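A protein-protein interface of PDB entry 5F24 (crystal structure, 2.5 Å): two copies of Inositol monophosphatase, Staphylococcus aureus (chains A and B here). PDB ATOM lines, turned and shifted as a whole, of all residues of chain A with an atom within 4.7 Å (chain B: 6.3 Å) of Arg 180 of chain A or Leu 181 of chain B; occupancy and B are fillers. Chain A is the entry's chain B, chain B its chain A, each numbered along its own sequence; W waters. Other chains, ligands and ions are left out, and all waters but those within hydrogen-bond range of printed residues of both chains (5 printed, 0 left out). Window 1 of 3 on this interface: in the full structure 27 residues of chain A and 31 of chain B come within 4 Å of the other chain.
Water W1 bridges O of Leu 181 of chain A (2.7 Å) and O of Leu 181 of chain B (3.3 Å).
Water W3 bridges the side-chain amide oxygen of Gln 162 of chain B (2.9 Å) and the backbone carbonyl oxygen of Tyr 179 of chain A (3.0 Å).
Water W2 lies within hydrogen-bond range of NH2 of Arg 180 of chain A (2.9 Å), NH2 of Arg 39 of chain B (3.2 Å) and OG of Ser 178 of chain A (3.3 Å).
Water W4 lies within hydrogen-bond range of the backbone carbonyl oxygen (O) of Gly 183 of chain B (2.9 Å), the backbone NH (N) of Asn 95 of chain B (2.9 Å) and the guanidinium group (NH1) of Arg 180 of chain A (3.2 Å).
Water W5 lies within hydrogen-bond range of N of Ser 178 of chain A (3.2 Å) and NE2 of Gln 162 of chain B (3.3 Å).
Tyr 179 of chain B touches its own counterpart, Tyr 179 of chain A.
Tyr 179 of chain A touches Leu 181 of chain B, and with the chains exchanged Leu 181 of chain A touches Tyr 179 of chain B.
Arg 180 of chain A touches Val 182 of chain B, and with the chains exchanged Val 182 of chain A touches Arg 180 of chain B.
Leu 181 of chain A touches its own counterpart, Leu 181 of chain B.
Of the 15 pairs that touch across the chains among the printed residues, 8 have their exchanged pair printed and touching as well.
Printed residues of chain A that touch a printed residue of chain B: Ile 156, Ser 178, Tyr 179, Arg 180, Leu 181, Val 182 and Phe 197.
Of the 20 printed residues of chain B, 9 touch a printed residue of chain A.
Among the printed residues, 15 pairs touch across the chains.
Among the printed residues, no Asp or Glu carboxylate lies within 4 Å of a Lys or Arg side-chain nitrogen of the other chain.
Of chain B, only Asn 95, Leu 181, Val 182 and Gly 183 come within 4 Å of Arg 180 of chain A.
Leu 181 of chain B touches just these residues of chain A: Tyr 179, Arg 180 and Leu 181.
Of the printed residues of chain B, Val 182 of chain A touches Arg 180.
Of the printed residues of chain A, Gly 183 of chain B touches Arg 180 (3.9 Å).
Printed residues of chain A within 4 Å of Tyr 179 of chain B: Tyr 179 and Leu 181.
Ala 161 of chain B touches none of the printed residues of chain A.
The nearest residue of chain B that does not touch Arg 180 of chain A is Gln 99 of chain B (4.1 Å).
The nearest printed residue of chain B that does not touch Phe 197 of chain A is Asn 95 of chain B (6.4 Å).
The side-chain amide oxygen of Asn 95 of chain B sits close to the side-chain amide oxygen of Gln 99 of chain B.
O of Asp 102 of chain B is in hydrogen-bond range of ND2 of Asn 95 of chain B.
O of Phe 159 of chain B sits at hydrogen-bond distance from OH of Tyr 179 of chain B, at 2.6 Å.
OD1 of Asn 160 of chain B is in hydrogen-bond range of N of Gln 162 of chain B.
The backbone NH (N) of Val 182 of chain B lies within hydrogen-bond range of the side-chain carboxylate (OD1) of Asp 188 of chain B (2.9 Å).
OD2 of Asp 188 of chain B lies within hydrogen-bond range of N of Gly 183 of chain B (2.8 Å).
Among the printed residues, pairs that only touch across the chains: Val 182 of chain A with Arg 180 of chain B, Phe 197 of chain A with Gln 99 of chain B, Arg 180 of chain A with Val 182 of chain B, Ser 178 of chain A with Gln 162 of chain B, Leu 181 of chain A with Tyr 179 of chain B, Tyr 179 of chain A with Tyr 179 of chain B, Tyr 179 of chain A with Leu 181 of chain B, Tyr 179 of chain A with Gln 162 of chain B, Leu 181 of chain A with Arg 180 of chain B, Arg 180 of chain A with Gly 183 of chain B, Arg 180 of chain A with Leu 181 of chain B and Ile 156 of chain A with Gln 99 of chain B.
NH1 of Arg 180 of chain A is in hydrogen-bond range of OD1 of Asn 95 of chain B.
N of Leu 181 of chain B sits at hydrogen-bond distance from O of Leu 181 of chain A.
OG of Ser 178 of chain A sits close to NH2 of Arg 39 of chain B, at 2.2 Å.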
ATOM      1  N   ILE A 156      10.565   9.249 -29.972  1.00  0.00           N
ATOM      2  CA  ILE A 156      10.700  10.043 -28.751  1.00  0.00           C
ATOM      3  C   ILE A 156       9.300  10.492 -28.386  1.00  0.00           C
ATOM      4  O   ILE A 156       8.576  10.838 -29.288  1.00  0.00           O
ATOM      5  CB  ILE A 156      11.626  11.227 -28.982  1.00  0.00           C
ATOM      6  CG1 ILE A 156      13.044  10.697 -29.038  1.00  0.00           C
ATOM      7  CG2 ILE A 156      11.457  12.245 -27.859  1.00  0.00           C
ATOM      8  CD1 ILE A 156      14.026  11.693 -29.589  1.00  0.00           C
ATOM      9  N   ILE A 157       8.906  10.463 -27.110  1.00  0.00           N
ATOM     10  CA  ILE A 157       7.619  11.061 -26.761  1.00  0.00           C
ATOM     11  C   ILE A 157       7.775  12.129 -25.729  1.00  0.00           C
ATOM     12  O   ILE A 157       8.752  12.188 -24.999  1.00  0.00           O
ATOM     13  CB  ILE A 157       6.533  10.062 -26.340  1.00  0.00           C
ATOM     14  CG1 ILE A 157       7.014   8.949 -25.418  1.00  0.00           C
ATOM     15  CG2 ILE A 157       6.122   9.268 -27.573  1.00  0.00           C
ATOM     16  CD1 ILE A 157       7.709   9.385 -24.185  1.00  0.00           C
ATOM     17  N   SER A 158       6.762  12.974 -25.704  1.00  0.00           N
ATOM     18  CA  SER A 158       6.782  14.191 -24.924  1.00  0.00           C
ATOM     19  C   SER A 158       5.432  14.326 -24.216  1.00  0.00           C
ATOM     20  O   SER A 158       4.369  14.233 -24.808  1.00  0.00           O
ATOM     21  CB  SER A 158       7.050  15.387 -25.838  1.00  0.00           C
ATOM     22  OG  SER A 158       6.681  16.620 -25.255  1.00  0.00           O
ATOM     23  N   PHE A 159       5.514  14.578 -22.908  1.00  0.00           N
ATOM     24  CA  PHE A 159       4.335  14.824 -22.105  1.00  0.00           C
ATOM     25  C   PHE A 159       4.794  15.337 -20.773  1.00  0.00           C
ATOM     26  O   PHE A 159       5.986  15.313 -20.479  1.00  0.00           O
ATOM     27  CB  PHE A 159       3.537  13.550 -21.918  1.00  0.00           C
ATOM     28  CG  PHE A 159       4.332  12.413 -21.337  1.00  0.00           C
ATOM     29  CD1 PHE A 159       5.000  11.518 -22.158  1.00  0.00           C
ATOM     30  CD2 PHE A 159       4.376  12.219 -19.965  1.00  0.00           C
ATOM     31  CE1 PHE A 159       5.688  10.445 -21.603  1.00  0.00           C
ATOM     32  CE2 PHE A 159       5.068  11.145 -19.419  1.00  0.00           C
ATOM     33  CZ  PHE A 159       5.726  10.261 -20.227  1.00  0.00           C
ATOM     34  N   SER A 178      12.689   7.103 -26.345  1.00  0.00           N
ATOM     35  CA  SER A 178      13.111   7.953 -25.258  1.00  0.00           C
ATOM     36  C   SER A 178      12.053   9.030 -24.947  1.00  0.00           C
ATOM     37  O   SER A 178      10.975   9.111 -25.586  1.00  0.00           O
ATOM     38  CB  SER A 178      14.475   8.581 -25.524  1.00  0.00           C
ATOM     39  OG  SER A 178      15.058   8.919 -24.294  1.00  0.00           O
ATOM     40  N   TYR A 179      12.367   9.887 -23.978  1.00  0.00           N
ATOM     41  CA  TYR A 179      11.452  10.916 -23.506  1.00  0.00           C
ATOM     42  C   TYR A 179      12.170  12.258 -23.567  1.00  0.00           C
ATOM     43  O   TYR A 179      13.335  12.365 -23.188  1.00  0.00           O
ATOM     44  CB  TYR A 179      11.054  10.610 -22.067  1.00  0.00           C
ATOM     45  CG  TYR A 179      10.296  11.721 -21.370  1.00  0.00           C
ATOM     46  CD1 TYR A 179       8.947  11.922 -21.570  1.00  0.00           C
ATOM     47  CD2 TYR A 179      10.942  12.595 -20.558  1.00  0.00           C
ATOM     48  CE1 TYR A 179       8.264  12.963 -20.934  1.00  0.00           C
ATOM     49  CE2 TYR A 179      10.293  13.654 -19.949  1.00  0.00           C
ATOM     50  CZ  TYR A 179       8.943  13.834 -20.106  1.00  0.00           C
ATOM     51  OH  TYR A 179       8.311  14.876 -19.416  1.00  0.00           O
ATOM     52  N   ARG A 180      11.469  13.284 -24.065  1.00  0.00           N
ATOM     53  CA  ARG A 180      11.954  14.660 -24.028  1.00  0.00           C
ATOM     54  C   ARG A 180      10.830  15.579 -23.716  1.00  0.00           C
ATOM     55  O   ARG A 180       9.670  15.231 -23.854  1.00  0.00           O
ATOM     56  CB  ARG A 180      12.623  15.214 -25.314  1.00  0.00           C
ATOM     57  CG  ARG A 180      13.616  14.371 -26.085  1.00  0.00           C
ATOM     58  CD  ARG A 180      15.091  14.571 -25.756  1.00  0.00           C
ATOM     59  NE  ARG A 180      15.451  13.376 -25.046  1.00  0.00           N
ATOM     60  CZ  ARG A 180      16.316  12.447 -25.395  1.00  0.00           C
ATOM     61  NH1 ARG A 180      17.117  12.526 -26.432  1.00  0.00           N
ATOM     62  NH2 ARG A 180      16.384  11.421 -24.605  1.00  0.00           N
ATOM     63  N   LEU A 181      11.181  16.785 -23.300  1.00  0.00           N
ATOM     64  CA  LEU A 181      10.180  17.842 -23.087  1.00  0.00           C
ATOM     65  C   LEU A 181      10.741  19.201 -23.406  1.00  0.00           C
ATOM     66  O   LEU A 181      11.664  19.685 -22.769  1.00  0.00           O
ATOM     67  CB  LEU A 181       9.670  17.834 -21.662  1.00  0.00           C
ATOM     68  CG  LEU A 181       8.505  18.796 -21.320  1.00  0.00           C
ATOM     69  CD1 LEU A 181       7.263  18.567 -22.173  1.00  0.00           C
ATOM     70  CD2 LEU A 181       8.124  18.636 -19.879  1.00  0.00           C
ATOM     71  N   VAL A 182      10.120  19.871 -24.376  1.00  0.00           N
ATOM     72  CA  VAL A 182      10.439  21.274 -24.687  1.00  0.00           C
ATOM     73  C   VAL A 182       9.743  22.195 -23.691  1.00  0.00           C
ATOM     74  O   VAL A 182      10.312  23.156 -23.249  1.00  0.00           O
ATOM     75  CB  VAL A 182      10.050  21.658 -26.107  1.00  0.00           C
ATOM     76  CG1 VAL A 182      10.384  23.121 -26.364  1.00  0.00           C
ATOM     77  CG2 VAL A 182      10.818  20.786 -27.095  1.00  0.00           C
ATOM     78  N   PHE A 197       9.404  14.054 -32.792  1.00  0.00           N
ATOM     79  CA  PHE A 197       8.747  13.284 -31.725  1.00  0.00           C
ATOM     80  C   PHE A 197       7.699  12.362 -32.374  1.00  0.00           C
ATOM     81  O   PHE A 197       7.108  12.760 -33.416  1.00  0.00           O
ATOM     82  CB  PHE A 197       8.030  14.261 -30.776  1.00  0.00           C
ATOM     83  CG  PHE A 197       8.942  15.088 -29.877  1.00  0.00           C
ATOM     84  CD1 PHE A 197      10.295  14.923 -29.849  1.00  0.00           C
ATOM     85  CD2 PHE A 197       8.384  16.009 -28.984  1.00  0.00           C
ATOM     86  CE1 PHE A 197      11.079  15.669 -28.969  1.00  0.00           C
ATOM     87  CE2 PHE A 197       9.166  16.759 -28.126  1.00  0.00           C
ATOM     88  CZ  PHE A 197      10.523  16.596 -28.122  1.00  0.00           C
ATOM     89  N   ARG B  39      18.070   2.984 -28.016  1.00  0.00           N
ATOM     90  CA  ARG B  39      18.875   4.103 -27.480  1.00  0.00           C
ATOM     91  C   ARG B  39      20.375   3.766 -27.357  1.00  0.00           C
ATOM     92  O   ARG B  39      21.230   4.581 -27.699  1.00  0.00           O
ATOM     93  CB  ARG B  39      18.285   4.528 -26.111  1.00  0.00           C
ATOM     94  CG  ARG B  39      18.718   5.878 -25.589  1.00  0.00           C
ATOM     95  CD  ARG B  39      18.882   5.895 -24.057  1.00  0.00           C
ATOM     96  NE  ARG B  39      17.723   5.365 -23.332  1.00  0.00           N
ATOM     97  CZ  ARG B  39      16.558   6.000 -23.125  1.00  0.00           C
ATOM     98  NH1 ARG B  39      15.586   5.416 -22.448  1.00  0.00           N
ATOM     99  NH2 ARG B  39      16.338   7.211 -23.584  1.00  0.00           N
ATOM    100  N   ALA B  94      21.274  10.389 -30.018  1.00  0.00           N
ATOM    101  CA  ALA B  94      19.871  10.024 -30.146  1.00  0.00           C
ATOM    102  C   ALA B  94      19.105  11.184 -30.757  1.00  0.00           C
ATOM    103  O   ALA B  94      18.348  10.980 -31.708  1.00  0.00           O
ATOM    104  CB  ALA B  94      19.285   9.649 -28.802  1.00  0.00           C
ATOM    105  N   ASN B  95      19.343  12.405 -30.254  1.00  0.00           N
ATOM    106  CA  ASN B  95      18.711  13.604 -30.835  1.00  0.00           C
ATOM    107  C   ASN B  95      19.152  13.865 -32.256  1.00  0.00           C
ATOM    108  O   ASN B  95      18.335  14.241 -33.080  1.00  0.00           O
ATOM    109  CB  ASN B  95      19.049  14.828 -30.027  1.00  0.00           C
ATOM    110  CG  ASN B  95      18.290  14.902 -28.745  1.00  0.00           C
ATOM    111  OD1 ASN B  95      17.297  14.223 -28.563  1.00  0.00           O
ATOM    112  ND2 ASN B  95      18.727  15.775 -27.856  1.00  0.00           N
ATOM    113  N   GLN B  99      15.999  13.578 -34.422  1.00  0.00           N
ATOM    114  CA  GLN B  99      15.494  14.950 -34.544  1.00  0.00           C
ATOM    115  C   GLN B  99      16.306  15.850 -35.429  1.00  0.00           C
ATOM    116  O   GLN B  99      15.805  16.885 -35.837  1.00  0.00           O
ATOM    117  CB  GLN B  99      15.415  15.626 -33.171  1.00  0.00           C
ATOM    118  CG  GLN B  99      14.720  14.827 -32.090  1.00  0.00           C
ATOM    119  CD  GLN B  99      14.303  15.722 -30.939  1.00  0.00           C
ATOM    120  OE1 GLN B  99      14.804  15.606 -29.813  1.00  0.00           O
ATOM    121  NE2 GLN B  99      13.411  16.627 -31.219  1.00  0.00           N
ATOM    122  N   ASP B 102      19.393  19.576 -31.442  1.00  0.00           N
ATOM    123  CA  ASP B 102      19.684  19.344 -29.988  1.00  0.00           C
ATOM    124  C   ASP B 102      20.800  18.344 -29.758  1.00  0.00           C
ATOM    125  O   ASP B 102      20.709  17.411 -28.933  1.00  0.00           O
ATOM    126  CB  ASP B 102      18.421  18.919 -29.178  1.00  0.00           C
ATOM    127  CG  ASP B 102      17.384  20.012 -29.117  1.00  0.00           C
ATOM    128  OD1 ASP B 102      17.778  21.185 -29.239  1.00  0.00           O
ATOM    129  OD2 ASP B 102      16.171  19.716 -28.930  1.00  0.00           O
ATOM    130  N   ILE B 157      14.654  22.023 -13.445  1.00  0.00           N
ATOM    131  CA  ILE B 157      15.754  21.066 -13.449  1.00  0.00           C
ATOM    132  C   ILE B 157      15.624  20.028 -14.514  1.00  0.00           C
ATOM    133  O   ILE B 157      14.545  19.813 -15.044  1.00  0.00           O
ATOM    134  CB  ILE B 157      15.977  20.362 -12.116  1.00  0.00           C
ATOM    135  CG1 ILE B 157      14.737  19.619 -11.669  1.00  0.00           C
ATOM    136  CG2 ILE B 157      16.498  21.401 -11.119  1.00  0.00           C
ATOM    137  CD1 ILE B 157      15.000  18.805 -10.424  1.00  0.00           C
ATOM    138  N   SER B 158      16.759  19.402 -14.793  1.00  0.00           N
ATOM    139  CA  SER B 158      16.913  18.513 -15.911  1.00  0.00           C
ATOM    140  C   SER B 158      17.719  17.296 -15.488  1.00  0.00           C
ATOM    141  O   SER B 158      18.752  17.374 -14.851  1.00  0.00           O
ATOM    142  CB  SER B 158      17.627  19.272 -17.050  1.00  0.00           C
ATOM    143  OG  SER B 158      18.186  18.417 -18.008  1.00  0.00           O
ATOM    144  N   PHE B 159      17.193  16.144 -15.871  1.00  0.00           N
ATOM    145  CA  PHE B 159      17.815  14.880 -15.583  1.00  0.00           C
ATOM    146  C   PHE B 159      17.070  13.815 -16.325  1.00  0.00           C
ATOM    147  O   PHE B 159      16.006  14.078 -16.865  1.00  0.00           O
ATOM    148  CB  PHE B 159      17.802  14.558 -14.080  1.00  0.00           C
ATOM    149  CG  PHE B 159      16.455  14.545 -13.474  1.00  0.00           C
ATOM    150  CD1 PHE B 159      15.683  13.368 -13.469  1.00  0.00           C
ATOM    151  CD2 PHE B 159      15.952  15.685 -12.852  1.00  0.00           C
ATOM    152  CE1 PHE B 159      14.427  13.354 -12.884  1.00  0.00           C
ATOM    153  CE2 PHE B 159      14.680  15.675 -12.282  1.00  0.00           C
ATOM    154  CZ  PHE B 159      13.928  14.514 -12.290  1.00  0.00           C
ATOM    155  N   ASN B 160      17.636  12.625 -16.392  1.00  0.00           N
ATOM    156  CA  ASN B 160      16.980  11.467 -17.011  1.00  0.00           C
ATOM    157  C   ASN B 160      16.133  10.781 -15.954  1.00  0.00           C
ATOM    158  O   ASN B 160      16.671  10.137 -15.046  1.00  0.00           O
ATOM    159  CB  ASN B 160      18.005  10.483 -17.567  1.00  0.00           C
ATOM    160  CG  ASN B 160      17.361   9.304 -18.284  1.00  0.00           C
ATOM    161  OD1 ASN B 160      16.164   9.120 -18.219  1.00  0.00           O
ATOM    162  ND2 ASN B 160      18.170   8.488 -18.956  1.00  0.00           N
ATOM    163  N   ALA B 161      14.820  10.887 -16.116  1.00  0.00           N
ATOM    164  CA  ALA B 161      13.895  10.331 -15.136  1.00  0.00           C
ATOM    165  C   ALA B 161      13.725   8.820 -15.252  1.00  0.00           C
ATOM    166  O   ALA B 161      12.986   8.254 -14.499  1.00  0.00           O
ATOM    167  CB  ALA B 161      12.537  10.971 -15.234  1.00  0.00           C
ATOM    168  N   GLN B 162      14.303   8.169 -16.266  1.00  0.00           N
ATOM    169  CA  GLN B 162      14.089   6.766 -16.552  1.00  0.00           C
ATOM    170  C   GLN B 162      15.056   5.917 -15.797  1.00  0.00           C
ATOM    171  O   GLN B 162      14.881   4.717 -15.710  1.00  0.00           O
ATOM    172  CB  GLN B 162      14.263   6.487 -18.043  1.00  0.00           C
ATOM    173  CG  GLN B 162      13.402   7.370 -18.923  1.00  0.00           C
ATOM    174  CD  GLN B 162      13.411   6.962 -20.382  1.00  0.00           C
ATOM    175  OE1 GLN B 162      13.766   7.756 -21.247  1.00  0.00           O
ATOM    176  NE2 GLN B 162      13.011   5.735 -20.669  1.00  0.00           N
ATOM    177  N   TYR B 179      10.302  20.810 -14.675  1.00  0.00           N
ATOM    178  CA  TYR B 179      11.225  19.829 -15.211  1.00  0.00           C
ATOM    179  C   TYR B 179      11.267  19.943 -16.746  1.00  0.00           C
ATOM    180  O   TYR B 179      10.210  20.063 -17.378  1.00  0.00           O
ATOM    181  CB  TYR B 179      10.776  18.421 -14.831  1.00  0.00           C
ATOM    182  CG  TYR B 179      11.514  17.293 -15.522  1.00  0.00           C
ATOM    183  CD1 TYR B 179      12.745  16.845 -15.065  1.00  0.00           C
ATOM    184  CD2 TYR B 179      10.985  16.700 -16.647  1.00  0.00           C
ATOM    185  CE1 TYR B 179      13.420  15.814 -15.700  1.00  0.00           C
ATOM    186  CE2 TYR B 179      11.642  15.670 -17.292  1.00  0.00           C
ATOM    187  CZ  TYR B 179      12.850  15.196 -16.815  1.00  0.00           C
ATOM    188  OH  TYR B 179      13.526  14.192 -17.525  1.00  0.00           O
ATOM    189  N   ARG B 180      12.481  19.980 -17.296  1.00  0.00           N
ATOM    190  CA  ARG B 180      12.655  19.912 -18.750  1.00  0.00           C
ATOM    191  C   ARG B 180      13.790  18.983 -19.068  1.00  0.00           C
ATOM    192  O   ARG B 180      14.593  18.658 -18.190  1.00  0.00           O
ATOM    193  CB  ARG B 180      12.962  21.250 -19.447  1.00  0.00           C
ATOM    194  CG  ARG B 180      12.175  22.490 -19.103  1.00  0.00           C
ATOM    195  CD  ARG B 180      10.952  22.788 -19.972  1.00  0.00           C
ATOM    196  NE  ARG B 180       9.838  22.511 -19.103  1.00  0.00           N
ATOM    197  CZ  ARG B 180       8.934  23.339 -18.615  1.00  0.00           C
ATOM    198  NH1 ARG B 180       8.807  24.591 -18.968  1.00  0.00           N
ATOM    199  NH2 ARG B 180       8.089  22.829 -17.785  1.00  0.00           N
ATOM    200  N   LEU B 181      13.855  18.573 -20.323  1.00  0.00           N
ATOM    201  CA  LEU B 181      15.004  17.805 -20.801  1.00  0.00           C
ATOM    202  C   LEU B 181      15.300  18.158 -22.246  1.00  0.00           C
ATOM    203  O   LEU B 181      14.492  17.908 -23.137  1.00  0.00           O
ATOM    204  CB  LEU B 181      14.763  16.308 -20.644  1.00  0.00           C
ATOM    205  CG  LEU B 181      15.931  15.375 -21.001  1.00  0.00           C
ATOM    206  CD1 LEU B 181      17.181  15.637 -20.201  1.00  0.00           C
ATOM    207  CD2 LEU B 181      15.520  13.931 -20.777  1.00  0.00           C
ATOM    208  N   VAL B 182      16.520  18.656 -22.497  1.00  0.00           N
ATOM    209  CA  VAL B 182      17.011  18.834 -23.855  1.00  0.00           C
ATOM    210  C   VAL B 182      17.510  17.513 -24.418  1.00  0.00           C
ATOM    211  O   VAL B 182      17.275  17.211 -25.567  1.00  0.00           O
ATOM    212  CB  VAL B 182      18.118  19.874 -23.944  1.00  0.00           C
ATOM    213  CG1 VAL B 182      18.596  20.004 -25.381  1.00  0.00           C
ATOM    214  CG2 VAL B 182      17.616  21.219 -23.444  1.00  0.00           C
ATOM    215  N   GLY B 183      18.232  16.744 -23.600  1.00  0.00           N
ATOM    216  CA  GLY B 183      18.620  15.379 -23.957  1.00  0.00           C
ATOM    217  C   GLY B 183      20.046  15.241 -24.468  1.00  0.00           C
ATOM    218  O   GLY B 183      20.395  14.236 -25.080  1.00  0.00           O
ATOM    219  N   ALA B 184      20.825  16.283 -24.330  1.00  0.00           N
ATOM    220  CA  ALA B 184      22.268  16.159 -24.559  1.00  0.00           C
ATOM    221  C   ALA B 184      22.989  16.740 -23.375  1.00  0.00           C
ATOM    222  O   ALA B 184      22.815  17.915 -23.081  1.00  0.00           O
ATOM    223  CB  ALA B 184      22.689  16.866 -25.822  1.00  0.00           C
ATOM    224  N   ASP B 188      22.119  20.459 -21.908  1.00  0.00           N
ATOM    225  CA  ASP B 188      21.467  20.601 -20.628  1.00  0.00           C
ATOM    226  C   ASP B 188      22.404  21.269 -19.621  1.00  0.00           C
ATOM    227  O   ASP B 188      21.971  22.106 -18.822  1.00  0.00           O
ATOM    228  CB  ASP B 188      21.026  19.244 -20.090  1.00  0.00           C
ATOM    229  CG  ASP B 188      19.825  18.664 -20.854  1.00  0.00           C
ATOM    230  OD1 ASP B 188      18.710  19.121 -20.605  1.00  0.00           O
ATOM    231  OD2 ASP B 188      19.989  17.712 -21.645  1.00  0.00           O
ATOM    232  N   PHE B 197      18.401  26.730 -16.442  1.00  0.00           N
ATOM    233  CA  PHE B 197      18.097  25.588 -15.555  1.00  0.00           C
ATOM    234  C   PHE B 197      18.871  25.839 -14.235  1.00  0.00           C
ATOM    235  O   PHE B 197      19.959  26.428 -14.247  1.00  0.00           O
ATOM    236  CB  PHE B 197      18.659  24.304 -16.201  1.00  0.00           C
ATOM    237  CG  PHE B 197      17.882  23.768 -17.381  1.00  0.00           C
ATOM    238  CD1 PHE B 197      16.751  24.377 -17.879  1.00  0.00           C
ATOM    239  CD2 PHE B 197      18.304  22.583 -17.980  1.00  0.00           C
ATOM    240  CE1 PHE B 197      16.065  23.841 -18.947  1.00  0.00           C
ATOM    241  CE2 PHE B 197      17.629  22.045 -19.062  1.00  0.00           C
ATOM    242  CZ  PHE B 197      16.492  22.677 -19.538  1.00  0.00           C
ATOM    243  N   HIS B 200      21.536  20.292 -13.698  1.00  0.00           N
ATOM    244  CA  HIS B 200      21.438  19.129 -14.549  1.00  0.00           C
ATOM    245  C   HIS B 200      22.132  17.967 -13.841  1.00  0.00           C
ATOM    246  O   HIS B 200      23.224  18.157 -13.277  1.00  0.00           O
ATOM    247  CB  HIS B 200      22.009  19.384 -15.950  1.00  0.00           C
ATOM    248  CG  HIS B 200      22.038  18.157 -16.803  1.00  0.00           C
ATOM    249  ND1 HIS B 200      20.891  17.520 -17.231  1.00  0.00           N
ATOM    250  CD2 HIS B 200      23.073  17.419 -17.271  1.00  0.00           C
ATOM    251  CE1 HIS B 200      21.217  16.459 -17.950  1.00  0.00           C
ATOM    252  NE2 HIS B 200      22.535  16.359 -17.968  1.00  0.00           N
HETATM  253  O   HOH W   1      13.886  21.161 -22.664  1.00  0.00           O
HETATM  254  O   HOH W   2      18.206   9.246 -25.120  1.00  0.00           O
HETATM  255  O   HOH W   3      14.454  10.518 -21.041  1.00  0.00           O
HETATM  256  O   HOH W   4      20.171  12.605 -27.460  1.00  0.00           O
HETATM  257  O   HOH W   5      11.616   5.999 -23.594  1.00  0.00           O
